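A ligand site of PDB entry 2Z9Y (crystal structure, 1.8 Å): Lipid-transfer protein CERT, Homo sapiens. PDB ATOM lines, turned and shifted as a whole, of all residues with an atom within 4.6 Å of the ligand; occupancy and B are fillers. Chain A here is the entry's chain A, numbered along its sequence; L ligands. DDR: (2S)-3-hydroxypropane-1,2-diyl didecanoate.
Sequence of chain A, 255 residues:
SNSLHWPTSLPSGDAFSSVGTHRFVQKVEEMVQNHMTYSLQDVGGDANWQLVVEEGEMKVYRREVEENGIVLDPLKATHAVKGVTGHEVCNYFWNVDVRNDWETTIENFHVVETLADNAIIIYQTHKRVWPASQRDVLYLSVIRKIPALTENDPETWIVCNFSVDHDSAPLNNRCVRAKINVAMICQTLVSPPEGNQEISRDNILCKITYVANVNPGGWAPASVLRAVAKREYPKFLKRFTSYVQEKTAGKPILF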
ATOM      1  N   PHE A  93      22.425 -31.872  18.385  1.00  0.00           N
ATOM      2  CA  PHE A  93      22.721 -30.441  18.391  1.00  0.00           C
ATOM      3  C   PHE A  93      21.553 -29.543  18.811  1.00  0.00           C
ATOM      4  O   PHE A  93      21.765 -28.496  19.453  1.00  0.00           O
ATOM      5  CB  PHE A  93      23.267 -30.026  16.996  1.00  0.00           C
ATOM      6  CG  PHE A  93      23.742 -28.603  16.942  1.00  0.00           C
ATOM      7  CD1 PHE A  93      24.931 -28.211  17.560  1.00  0.00           C
ATOM      8  CD2 PHE A  93      23.005 -27.658  16.256  1.00  0.00           C
ATOM      9  CE1 PHE A  93      25.375 -26.869  17.490  1.00  0.00           C
ATOM     10  CE2 PHE A  93      23.434 -26.316  16.195  1.00  0.00           C
ATOM     11  CZ  PHE A  93      24.625 -25.938  16.816  1.00  0.00           C
ATOM     12  N   ARG A  99      21.581 -30.696  25.937  1.00  0.00           N
ATOM     13  CA  ARG A  99      22.515 -29.592  25.814  1.00  0.00           C
ATOM     14  C   ARG A  99      23.669 -29.631  26.816  1.00  0.00           C
ATOM     15  O   ARG A  99      24.814 -29.496  26.434  1.00  0.00           O
ATOM     16  CB  ARG A  99      21.770 -28.252  25.914  1.00  0.00           C
ATOM     17  CG  ARG A  99      22.655 -27.034  25.594  1.00  0.00           C
ATOM     18  CD  ARG A  99      22.872 -26.872  24.105  1.00  0.00           C
ATOM     19  NE  ARG A  99      21.897 -25.940  23.549  1.00  0.00           N
ATOM     20  CZ  ARG A  99      20.984 -26.232  22.631  1.00  0.00           C
ATOM     21  NH1 ARG A  99      20.894 -27.447  22.115  1.00  0.00           N
ATOM     22  NH2 ARG A  99      20.158 -25.280  22.233  1.00  0.00           N
ATOM     23  N   TRP A 102      26.911 -31.925  26.692  1.00  0.00           N
ATOM     24  CA  TRP A 102      28.069 -31.625  25.809  1.00  0.00           C
ATOM     25  C   TRP A 102      28.543 -30.171  25.789  1.00  0.00           C
ATOM     26  O   TRP A 102      29.714 -29.895  25.460  1.00  0.00           O
ATOM     27  CB  TRP A 102      27.835 -32.150  24.374  1.00  0.00           C
ATOM     28  CG  TRP A 102      26.639 -31.559  23.704  1.00  0.00           C
ATOM     29  CD1 TRP A 102      25.385 -32.079  23.645  1.00  0.00           C
ATOM     30  CD2 TRP A 102      26.607 -30.315  22.991  1.00  0.00           C
ATOM     31  NE1 TRP A 102      24.555 -31.229  22.950  1.00  0.00           N
ATOM     32  CE2 TRP A 102      25.280 -30.141  22.537  1.00  0.00           C
ATOM     33  CE3 TRP A 102      27.557 -29.321  22.710  1.00  0.00           C
ATOM     34  CZ2 TRP A 102      24.878 -29.006  21.806  1.00  0.00           C
ATOM     35  CZ3 TRP A 102      27.164 -28.194  21.971  1.00  0.00           C
ATOM     36  CH2 TRP A 102      25.825 -28.048  21.532  1.00  0.00           C
ATOM     37  N   GLU A 103      27.658 -29.229  26.098  1.00  0.00           N
ATOM     38  CA  GLU A 103      28.034 -27.809  26.023  1.00  0.00           C
ATOM     39  C   GLU A 103      28.781 -27.304  27.265  1.00  0.00           C
ATOM     40  O   GLU A 103      28.409 -27.625  28.390  1.00  0.00           O
ATOM     41  CB  GLU A 103      26.791 -26.954  25.794  1.00  0.00           C
ATOM     42  CG  GLU A 103      27.040 -25.450  26.066  1.00  0.00           C
ATOM     43  CD  GLU A 103      27.628 -24.786  24.857  1.00  0.00           C
ATOM     44  OE1 GLU A 103      26.963 -24.870  23.796  1.00  0.00           O
ATOM     45  OE2 GLU A 103      28.721 -24.212  24.947  1.00  0.00           O
ATOM     46  N   THR A 105      30.190 -23.732  27.436  1.00  0.00           N
ATOM     47  CA  THR A 105      30.221 -22.269  27.558  1.00  0.00           C
ATOM     48  C   THR A 105      28.914 -21.636  28.044  1.00  0.00           C
ATOM     49  O   THR A 105      28.842 -20.422  28.190  1.00  0.00           O
ATOM     50  CB  THR A 105      30.556 -21.605  26.206  1.00  0.00           C
ATOM     51  OG1 THR A 105      29.379 -21.612  25.387  1.00  0.00           O
ATOM     52  CG2 THR A 105      31.661 -22.340  25.493  1.00  0.00           C
ATOM     53  N   GLN A 124      19.631 -17.589  26.435  1.00  0.00           N
ATOM     54  CA  GLN A 124      20.757 -18.139  27.190  1.00  0.00           C
ATOM     55  C   GLN A 124      21.833 -17.137  27.602  1.00  0.00           C
ATOM     56  O   GLN A 124      22.103 -16.153  26.902  1.00  0.00           O
ATOM     57  CB  GLN A 124      21.413 -19.319  26.443  1.00  0.00           C
ATOM     58  CG  GLN A 124      22.291 -18.903  25.273  1.00  0.00           C
ATOM     59  CD  GLN A 124      22.690 -20.055  24.377  1.00  0.00           C
ATOM     60  OE1 GLN A 124      22.023 -21.094  24.361  1.00  0.00           O
ATOM     61  NE2 GLN A 124      23.763 -19.880  23.595  1.00  0.00           N
ATOM     62  N   HIS A 126      25.925 -16.834  28.799  1.00  0.00           N
ATOM     63  CA  HIS A 126      27.185 -17.517  28.701  1.00  0.00           C
ATOM     64  C   HIS A 126      28.082 -17.237  29.910  1.00  0.00           C
ATOM     65  O   HIS A 126      27.986 -16.182  30.524  1.00  0.00           O
ATOM     66  CB  HIS A 126      27.896 -17.114  27.412  1.00  0.00           C
ATOM     67  CG  HIS A 126      27.269 -17.711  26.184  1.00  0.00           C
ATOM     68  ND1 HIS A 126      27.679 -18.912  25.651  1.00  0.00           N
ATOM     69  CD2 HIS A 126      26.220 -17.310  25.442  1.00  0.00           C
ATOM     70  CE1 HIS A 126      26.936 -19.202  24.598  1.00  0.00           C
ATOM     71  NE2 HIS A 126      26.030 -18.255  24.459  1.00  0.00           N
ATOM     72  N   VAL A 129      33.698 -16.290  28.866  1.00  0.00           N
ATOM     73  CA  VAL A 129      34.679 -16.983  28.025  1.00  0.00           C
ATOM     74  C   VAL A 129      35.913 -16.144  27.688  1.00  0.00           C
ATOM     75  O   VAL A 129      36.998 -16.682  27.464  1.00  0.00           O
ATOM     76  CB  VAL A 129      34.028 -17.584  26.733  1.00  0.00           C
ATOM     77  CG1 VAL A 129      33.378 -18.935  27.050  1.00  0.00           C
ATOM     78  CG2 VAL A 129      33.004 -16.633  26.126  1.00  0.00           C
ATOM     79  N   TRP A 130      35.736 -14.824  27.632  1.00  0.00           N
ATOM     80  CA  TRP A 130      36.882 -13.911  27.702  1.00  0.00           C
ATOM     81  C   TRP A 130      36.657 -12.934  28.876  1.00  0.00           C
ATOM     82  O   TRP A 130      35.524 -12.811  29.345  1.00  0.00           O
ATOM     83  CB  TRP A 130      37.112 -13.186  26.385  1.00  0.00           C
ATOM     84  CG  TRP A 130      36.050 -12.211  26.016  1.00  0.00           C
ATOM     85  CD1 TRP A 130      35.996 -10.893  26.368  1.00  0.00           C
ATOM     86  CD2 TRP A 130      34.917 -12.460  25.175  1.00  0.00           C
ATOM     87  NE1 TRP A 130      34.890 -10.304  25.823  1.00  0.00           N
ATOM     88  CE2 TRP A 130      34.198 -11.242  25.090  1.00  0.00           C
ATOM     89  CE3 TRP A 130      34.426 -13.587  24.499  1.00  0.00           C
ATOM     90  CZ2 TRP A 130      33.019 -11.124  24.335  1.00  0.00           C
ATOM     91  CZ3 TRP A 130      33.245 -13.464  23.763  1.00  0.00           C
ATOM     92  CH2 TRP A 130      32.560 -12.246  23.692  1.00  0.00           C
ATOM     93  N   ARG A 135      27.965 -12.282  28.076  1.00  0.00           N
ATOM     94  CA  ARG A 135      26.959 -12.057  27.038  1.00  0.00           C
ATOM     95  C   ARG A 135      25.748 -12.951  27.287  1.00  0.00           C
ATOM     96  O   ARG A 135      25.880 -14.083  27.810  1.00  0.00           O
ATOM     97  CB  ARG A 135      27.472 -12.286  25.602  1.00  0.00           C
ATOM     98  CG  ARG A 135      28.894 -11.831  25.314  1.00  0.00           C
ATOM     99  CD  ARG A 135      29.063 -10.331  25.185  1.00  0.00           C
ATOM    100  NE  ARG A 135      30.187  -9.901  25.993  1.00  0.00           N
ATOM    101  CZ  ARG A 135      30.915  -8.811  25.797  1.00  0.00           C
ATOM    102  NH1 ARG A 135      30.677  -7.997  24.777  1.00  0.00           N
ATOM    103  NH2 ARG A 135      31.901  -8.537  26.635  1.00  0.00           N
ATOM    104  N   TYR A 139      17.601 -16.479  20.684  1.00  0.00           N
ATOM    105  CA  TYR A 139      17.628 -16.958  19.310  1.00  0.00           C
ATOM    106  C   TYR A 139      16.531 -17.967  19.000  1.00  0.00           C
ATOM    107  O   TYR A 139      16.048 -18.681  19.892  1.00  0.00           O
ATOM    108  CB  TYR A 139      19.016 -17.543  18.978  1.00  0.00           C
ATOM    109  CG  TYR A 139      19.487 -18.749  19.775  1.00  0.00           C
ATOM    110  CD1 TYR A 139      19.342 -20.046  19.282  1.00  0.00           C
ATOM    111  CD2 TYR A 139      20.105 -18.590  21.020  1.00  0.00           C
ATOM    112  CE1 TYR A 139      19.816 -21.176  20.000  1.00  0.00           C
ATOM    113  CE2 TYR A 139      20.565 -19.682  21.748  1.00  0.00           C
ATOM    114  CZ  TYR A 139      20.428 -20.975  21.234  1.00  0.00           C
ATOM    115  OH  TYR A 139      20.903 -22.026  21.975  1.00  0.00           O
ATOM    116  N   SER A 141      15.812 -21.458  17.311  1.00  0.00           N
ATOM    117  CA  SER A 141      16.527 -22.703  16.989  1.00  0.00           C
ATOM    118  C   SER A 141      15.561 -23.652  16.288  1.00  0.00           C
ATOM    119  O   SER A 141      14.578 -24.103  16.885  1.00  0.00           O
ATOM    120  CB  SER A 141      17.123 -23.315  18.264  1.00  0.00           C
ATOM    121  OG  SER A 141      17.918 -24.471  18.024  1.00  0.00           O
ATOM    122  N   ASN A 161      20.386 -21.645  14.071  1.00  0.00           N
ATOM    123  CA  ASN A 161      20.196 -20.831  15.276  1.00  0.00           C
ATOM    124  C   ASN A 161      20.445 -19.373  14.940  1.00  0.00           C
ATOM    125  O   ASN A 161      21.581 -19.035  14.583  1.00  0.00           O
ATOM    126  CB  ASN A 161      21.149 -21.287  16.382  1.00  0.00           C
ATOM    127  CG  ASN A 161      20.855 -22.728  16.874  1.00  0.00           C
ATOM    128  OD1 ASN A 161      19.764 -23.253  16.681  1.00  0.00           O
ATOM    129  ND2 ASN A 161      21.871 -23.366  17.471  1.00  0.00           N
ATOM    130  N   ALA A 178      24.732 -10.497  22.597  1.00  0.00           N
ATOM    131  CA  ALA A 178      25.352 -10.977  21.344  1.00  0.00           C
ATOM    132  C   ALA A 178      24.291 -11.249  20.280  1.00  0.00           C
ATOM    133  O   ALA A 178      23.140 -11.527  20.622  1.00  0.00           O
ATOM    134  CB  ALA A 178      26.175 -12.227  21.604  1.00  0.00           C
ATOM    135  N   ILE A 180      23.672 -13.735  16.895  1.00  0.00           N
ATOM    136  CA  ILE A 180      24.241 -14.921  16.253  1.00  0.00           C
ATOM    137  C   ILE A 180      23.489 -15.334  15.000  1.00  0.00           C
ATOM    138  O   ILE A 180      22.281 -15.093  14.885  1.00  0.00           O
ATOM    139  CB  ILE A 180      24.343 -16.109  17.220  1.00  0.00           C
ATOM    140  CG1 ILE A 180      22.932 -16.647  17.529  1.00  0.00           C
ATOM    141  CG2 ILE A 180      25.149 -15.724  18.486  1.00  0.00           C
ATOM    142  CD1 ILE A 180      22.935 -17.996  18.335  1.00  0.00           C
ATOM    143  N   VAL A 182      24.033 -19.026  13.299  1.00  0.00           N
ATOM    144  CA  VAL A 182      24.793 -20.277  13.377  1.00  0.00           C
ATOM    145  C   VAL A 182      24.047 -21.369  12.610  1.00  0.00           C
ATOM    146  O   VAL A 182      22.806 -21.407  12.597  1.00  0.00           O
ATOM    147  CB  VAL A 182      24.991 -20.708  14.903  1.00  0.00           C
ATOM    148  CG1 VAL A 182      25.508 -22.144  15.036  1.00  0.00           C
ATOM    149  CG2 VAL A 182      25.945 -19.786  15.620  1.00  0.00           C
ATOM    150  N   TYR A 210      29.727 -26.564   9.856  1.00  0.00           N
ATOM    151  CA  TYR A 210      29.274 -25.761  10.971  1.00  0.00           C
ATOM    152  C   TYR A 210      29.680 -24.317  10.676  1.00  0.00           C
ATOM    153  O   TYR A 210      30.865 -24.062  10.468  1.00  0.00           O
ATOM    154  CB  TYR A 210      29.946 -26.203  12.246  1.00  0.00           C
ATOM    155  CG  TYR A 210      29.620 -25.326  13.421  1.00  0.00           C
ATOM    156  CD1 TYR A 210      28.422 -25.469  14.098  1.00  0.00           C
ATOM    157  CD2 TYR A 210      30.541 -24.361  13.876  1.00  0.00           C
ATOM    158  CE1 TYR A 210      28.109 -24.636  15.202  1.00  0.00           C
ATOM    159  CE2 TYR A 210      30.227 -23.518  14.967  1.00  0.00           C
ATOM    160  CZ  TYR A 210      29.025 -23.673  15.625  1.00  0.00           C
ATOM    161  OH  TYR A 210      28.708 -22.844  16.689  1.00  0.00           O
ATOM    162  N   VAL A 214      29.003 -14.391  14.564  1.00  0.00           N
ATOM    163  CA  VAL A 214      28.652 -13.859  15.867  1.00  0.00           C
ATOM    164  C   VAL A 214      29.092 -12.409  15.999  1.00  0.00           C
ATOM    165  O   VAL A 214      30.212 -12.048  15.625  1.00  0.00           O
ATOM    166  CB  VAL A 214      29.308 -14.684  16.961  1.00  0.00           C
ATOM    167  CG1 VAL A 214      29.009 -14.068  18.343  1.00  0.00           C
ATOM    168  CG2 VAL A 214      28.833 -16.125  16.884  1.00  0.00           C
ATOM    169  N   VAL A 228      40.037 -16.744  21.660  1.00  0.00           N
ATOM    170  CA  VAL A 228      38.929 -17.470  22.337  1.00  0.00           C
ATOM    171  C   VAL A 228      38.196 -18.331  21.281  1.00  0.00           C
ATOM    172  O   VAL A 228      37.910 -19.521  21.501  1.00  0.00           O
ATOM    173  CB  VAL A 228      37.955 -16.503  23.064  1.00  0.00           C
ATOM    174  CG1 VAL A 228      36.659 -17.206  23.476  1.00  0.00           C
ATOM    175  CG2 VAL A 228      38.604 -15.859  24.294  1.00  0.00           C
ATOM    176  N   GLU A 232      37.651 -22.230  21.525  1.00  0.00           N
ATOM    177  CA  GLU A 232      36.321 -22.742  21.930  1.00  0.00           C
ATOM    178  C   GLU A 232      35.556 -23.496  20.815  1.00  0.00           C
ATOM    179  O   GLU A 232      34.817 -24.452  21.082  1.00  0.00           O
ATOM    180  CB  GLU A 232      35.455 -21.617  22.468  1.00  0.00           C
ATOM    181  CG  GLU A 232      35.954 -21.022  23.784  1.00  0.00           C
ATOM    182  CD  GLU A 232      35.982 -22.039  24.919  1.00  0.00           C
ATOM    183  OE1 GLU A 232      35.056 -22.875  24.992  1.00  0.00           O
ATOM    184  OE2 GLU A 232      36.940 -22.003  25.726  1.00  0.00           O
ATOM    185  N   TYR A 233      35.708 -23.059  19.555  1.00  0.00           N
ATOM    186  CA  TYR A 233      35.022 -23.793  18.486  1.00  0.00           C
ATOM    187  C   TYR A 233      35.526 -25.220  18.243  1.00  0.00           C
ATOM    188  O   TYR A 233      34.701 -26.149  18.215  1.00  0.00           O
ATOM    189  CB  TYR A 233      34.964 -22.967  17.185  1.00  0.00           C
ATOM    190  CG  TYR A 233      34.008 -21.787  17.245  1.00  0.00           C
ATOM    191  CD1 TYR A 233      34.502 -20.467  17.299  1.00  0.00           C
ATOM    192  CD2 TYR A 233      32.613 -21.967  17.267  1.00  0.00           C
ATOM    193  CE1 TYR A 233      33.632 -19.369  17.337  1.00  0.00           C
ATOM    194  CE2 TYR A 233      31.744 -20.872  17.295  1.00  0.00           C
ATOM    195  CZ  TYR A 233      32.264 -19.574  17.337  1.00  0.00           C
ATOM    196  OH  TYR A 233      31.416 -18.483  17.369  1.00  0.00           O
ATOM    197  N   PHE A 236      34.528 -27.457  21.201  1.00  0.00           N
ATOM    198  CA  PHE A 236      33.113 -27.818  21.004  1.00  0.00           C
ATOM    199  C   PHE A 236      32.944 -28.918  19.946  1.00  0.00           C
ATOM    200  O   PHE A 236      32.345 -29.936  20.192  1.00  0.00           O
ATOM    201  CB  PHE A 236      32.277 -26.554  20.688  1.00  0.00           C
ATOM    202  CG  PHE A 236      31.164 -26.789  19.681  1.00  0.00           C
ATOM    203  CD1 PHE A 236      30.085 -27.601  19.989  1.00  0.00           C
ATOM    204  CD2 PHE A 236      31.243 -26.224  18.383  1.00  0.00           C
ATOM    205  CE1 PHE A 236      29.077 -27.870  19.064  1.00  0.00           C
ATOM    206  CE2 PHE A 236      30.219 -26.472  17.432  1.00  0.00           C
ATOM    207  CZ  PHE A 236      29.124 -27.291  17.780  1.00  0.00           C
HETATM  208  O21 DDR L   1      26.616 -23.623  18.419  1.00  0.00           O
HETATM  209  C21 DDR L   1      26.632 -24.227  19.509  1.00  0.00           C
HETATM  210  C22 DDR L   1      27.918 -24.635  20.167  1.00  0.00           C
HETATM  211  C23 DDR L   1      28.982 -23.552  20.075  1.00  0.00           C
HETATM  212  C24 DDR L   1      29.676 -23.337  21.419  1.00  0.00           C
HETATM  213  C25 DDR L   1      31.024 -22.640  21.252  1.00  0.00           C
HETATM  214  C26 DDR L   1      30.837 -21.138  21.164  1.00  0.00           C
HETATM  215  C27 DDR L   1      32.138 -20.422  21.524  1.00  0.00           C
HETATM  216  C28 DDR L   1      31.929 -18.926  21.631  1.00  0.00           C
HETATM  217  C29 DDR L   1      33.272 -18.230  21.526  1.00  0.00           C
HETATM  218  C30 DDR L   1      33.152 -16.868  20.889  1.00  0.00           C
HETATM  219  O52 DDR L   1      25.427 -24.612  20.251  1.00  0.00           O
HETATM  220  C52 DDR L   1      24.113 -24.312  19.770  1.00  0.00           C
HETATM  221  C53 DDR L   1      23.233 -25.558  19.911  1.00  0.00           C
HETATM  222  O53 DDR L   1      22.045 -25.492  19.095  1.00  0.00           O
HETATM  223  C51 DDR L   1      23.526 -23.253  20.676  1.00  0.00           C
HETATM  224  O51 DDR L   1      24.428 -22.146  20.765  1.00  0.00           O
HETATM  225  C1  DDR L   1      24.529 -21.282  19.629  1.00  0.00           C
HETATM  226  O1  DDR L   1      23.908 -21.547  18.615  1.00  0.00           O
HETATM  227  C2  DDR L   1      25.386 -20.040  19.692  1.00  0.00           C
HETATM  228  C3  DDR L   1      26.850 -20.439  19.666  1.00  0.00           C
HETATM  229  C4  DDR L   1      27.724 -19.200  19.526  1.00  0.00           C
HETATM  230  C5  DDR L   1      27.725 -18.444  20.850  1.00  0.00           C
HETATM  231  C6  DDR L   1      28.483 -17.130  20.689  1.00  0.00           C
HETATM  232  C7  DDR L   1      27.998 -16.077  21.671  1.00  0.00           C
HETATM  233  C8  DDR L   1      29.144 -15.252  22.225  1.00  0.00           C
HETATM  234  C9  DDR L   1      29.756 -16.006  23.390  1.00  0.00           C
HETATM  235  C10 DDR L   1      29.439 -15.312  24.680  1.00  0.00           C
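The side-chain amide nitrogen (ND2) of Asn 161 sits at hydrogen-bond distance from an oxygen (O53) of the ligand, at 2.7 Å.
The side-chain hydroxyl (OH) of Tyr 210 sits at hydrogen-bond distance from an oxygen (O21) of the ligand.
The backbone carbonyl oxygen (O) of Phe 93 is in hydrogen-bond range of an oxygen (O53) of the ligand.
The side-chain amide oxygen (OD1) of Asn 161 is in hydrogen-bond range of the side-chain hydroxyl (OG) of Ser 141 (2.6 Å).
NH1 of Arg 99 sits at hydrogen-bond distance from O of Phe 93, 3.0 Å away.
OH of Tyr 139 lies within hydrogen-bond range of NH2 of Arg 99, at 3.3 Å.
The side-chain amide oxygen (OE1) of Gln 124 lies within hydrogen-bond range of the side-chain hydroxyl (OH) of Tyr 139.
O of Arg 135 sits at hydrogen-bond distance from N of His 126 (2.9 Å).
A ring nitrogen (NE2) of His 126 sits at hydrogen-bond distance from the side-chain amide nitrogen (NE2) of Gln 124.
The backbone carbonyl oxygen (O) of Thr 105 lies within hydrogen-bond range of a ring nitrogen (ND1) of His 126 (3.2 Å).
The side-chain hydroxyl (OG1) of Thr 105 lies within hydrogen-bond range of the side-chain carboxylate (OE2) of Glu 103, at 2.7 Å.
Residues that only touch the ligand: Arg 99, Trp 102, Glu 103, Gln 124, His 126, Arg 135, Tyr 139, Ile 180, Val 182, Val 214, Glu 232, Tyr 233 and Phe 236.
Hydrophobic or aromatic side chains that line the ligand: Phe 93, Trp 102, His 126, Tyr 139, Ile 180, Val 182, Tyr 210, Val 214, Tyr 233 and Phe 236.
16 residues have an atom within 4 Å of the ligand: Phe 93, Arg 99, Trp 102, Glu 103, Gln 124, His 126, Arg 135, Tyr 139, Asn 161, Ile 180, Val 182, Tyr 210, Val 214, Glu 232, Tyr 233 and Phe 236.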
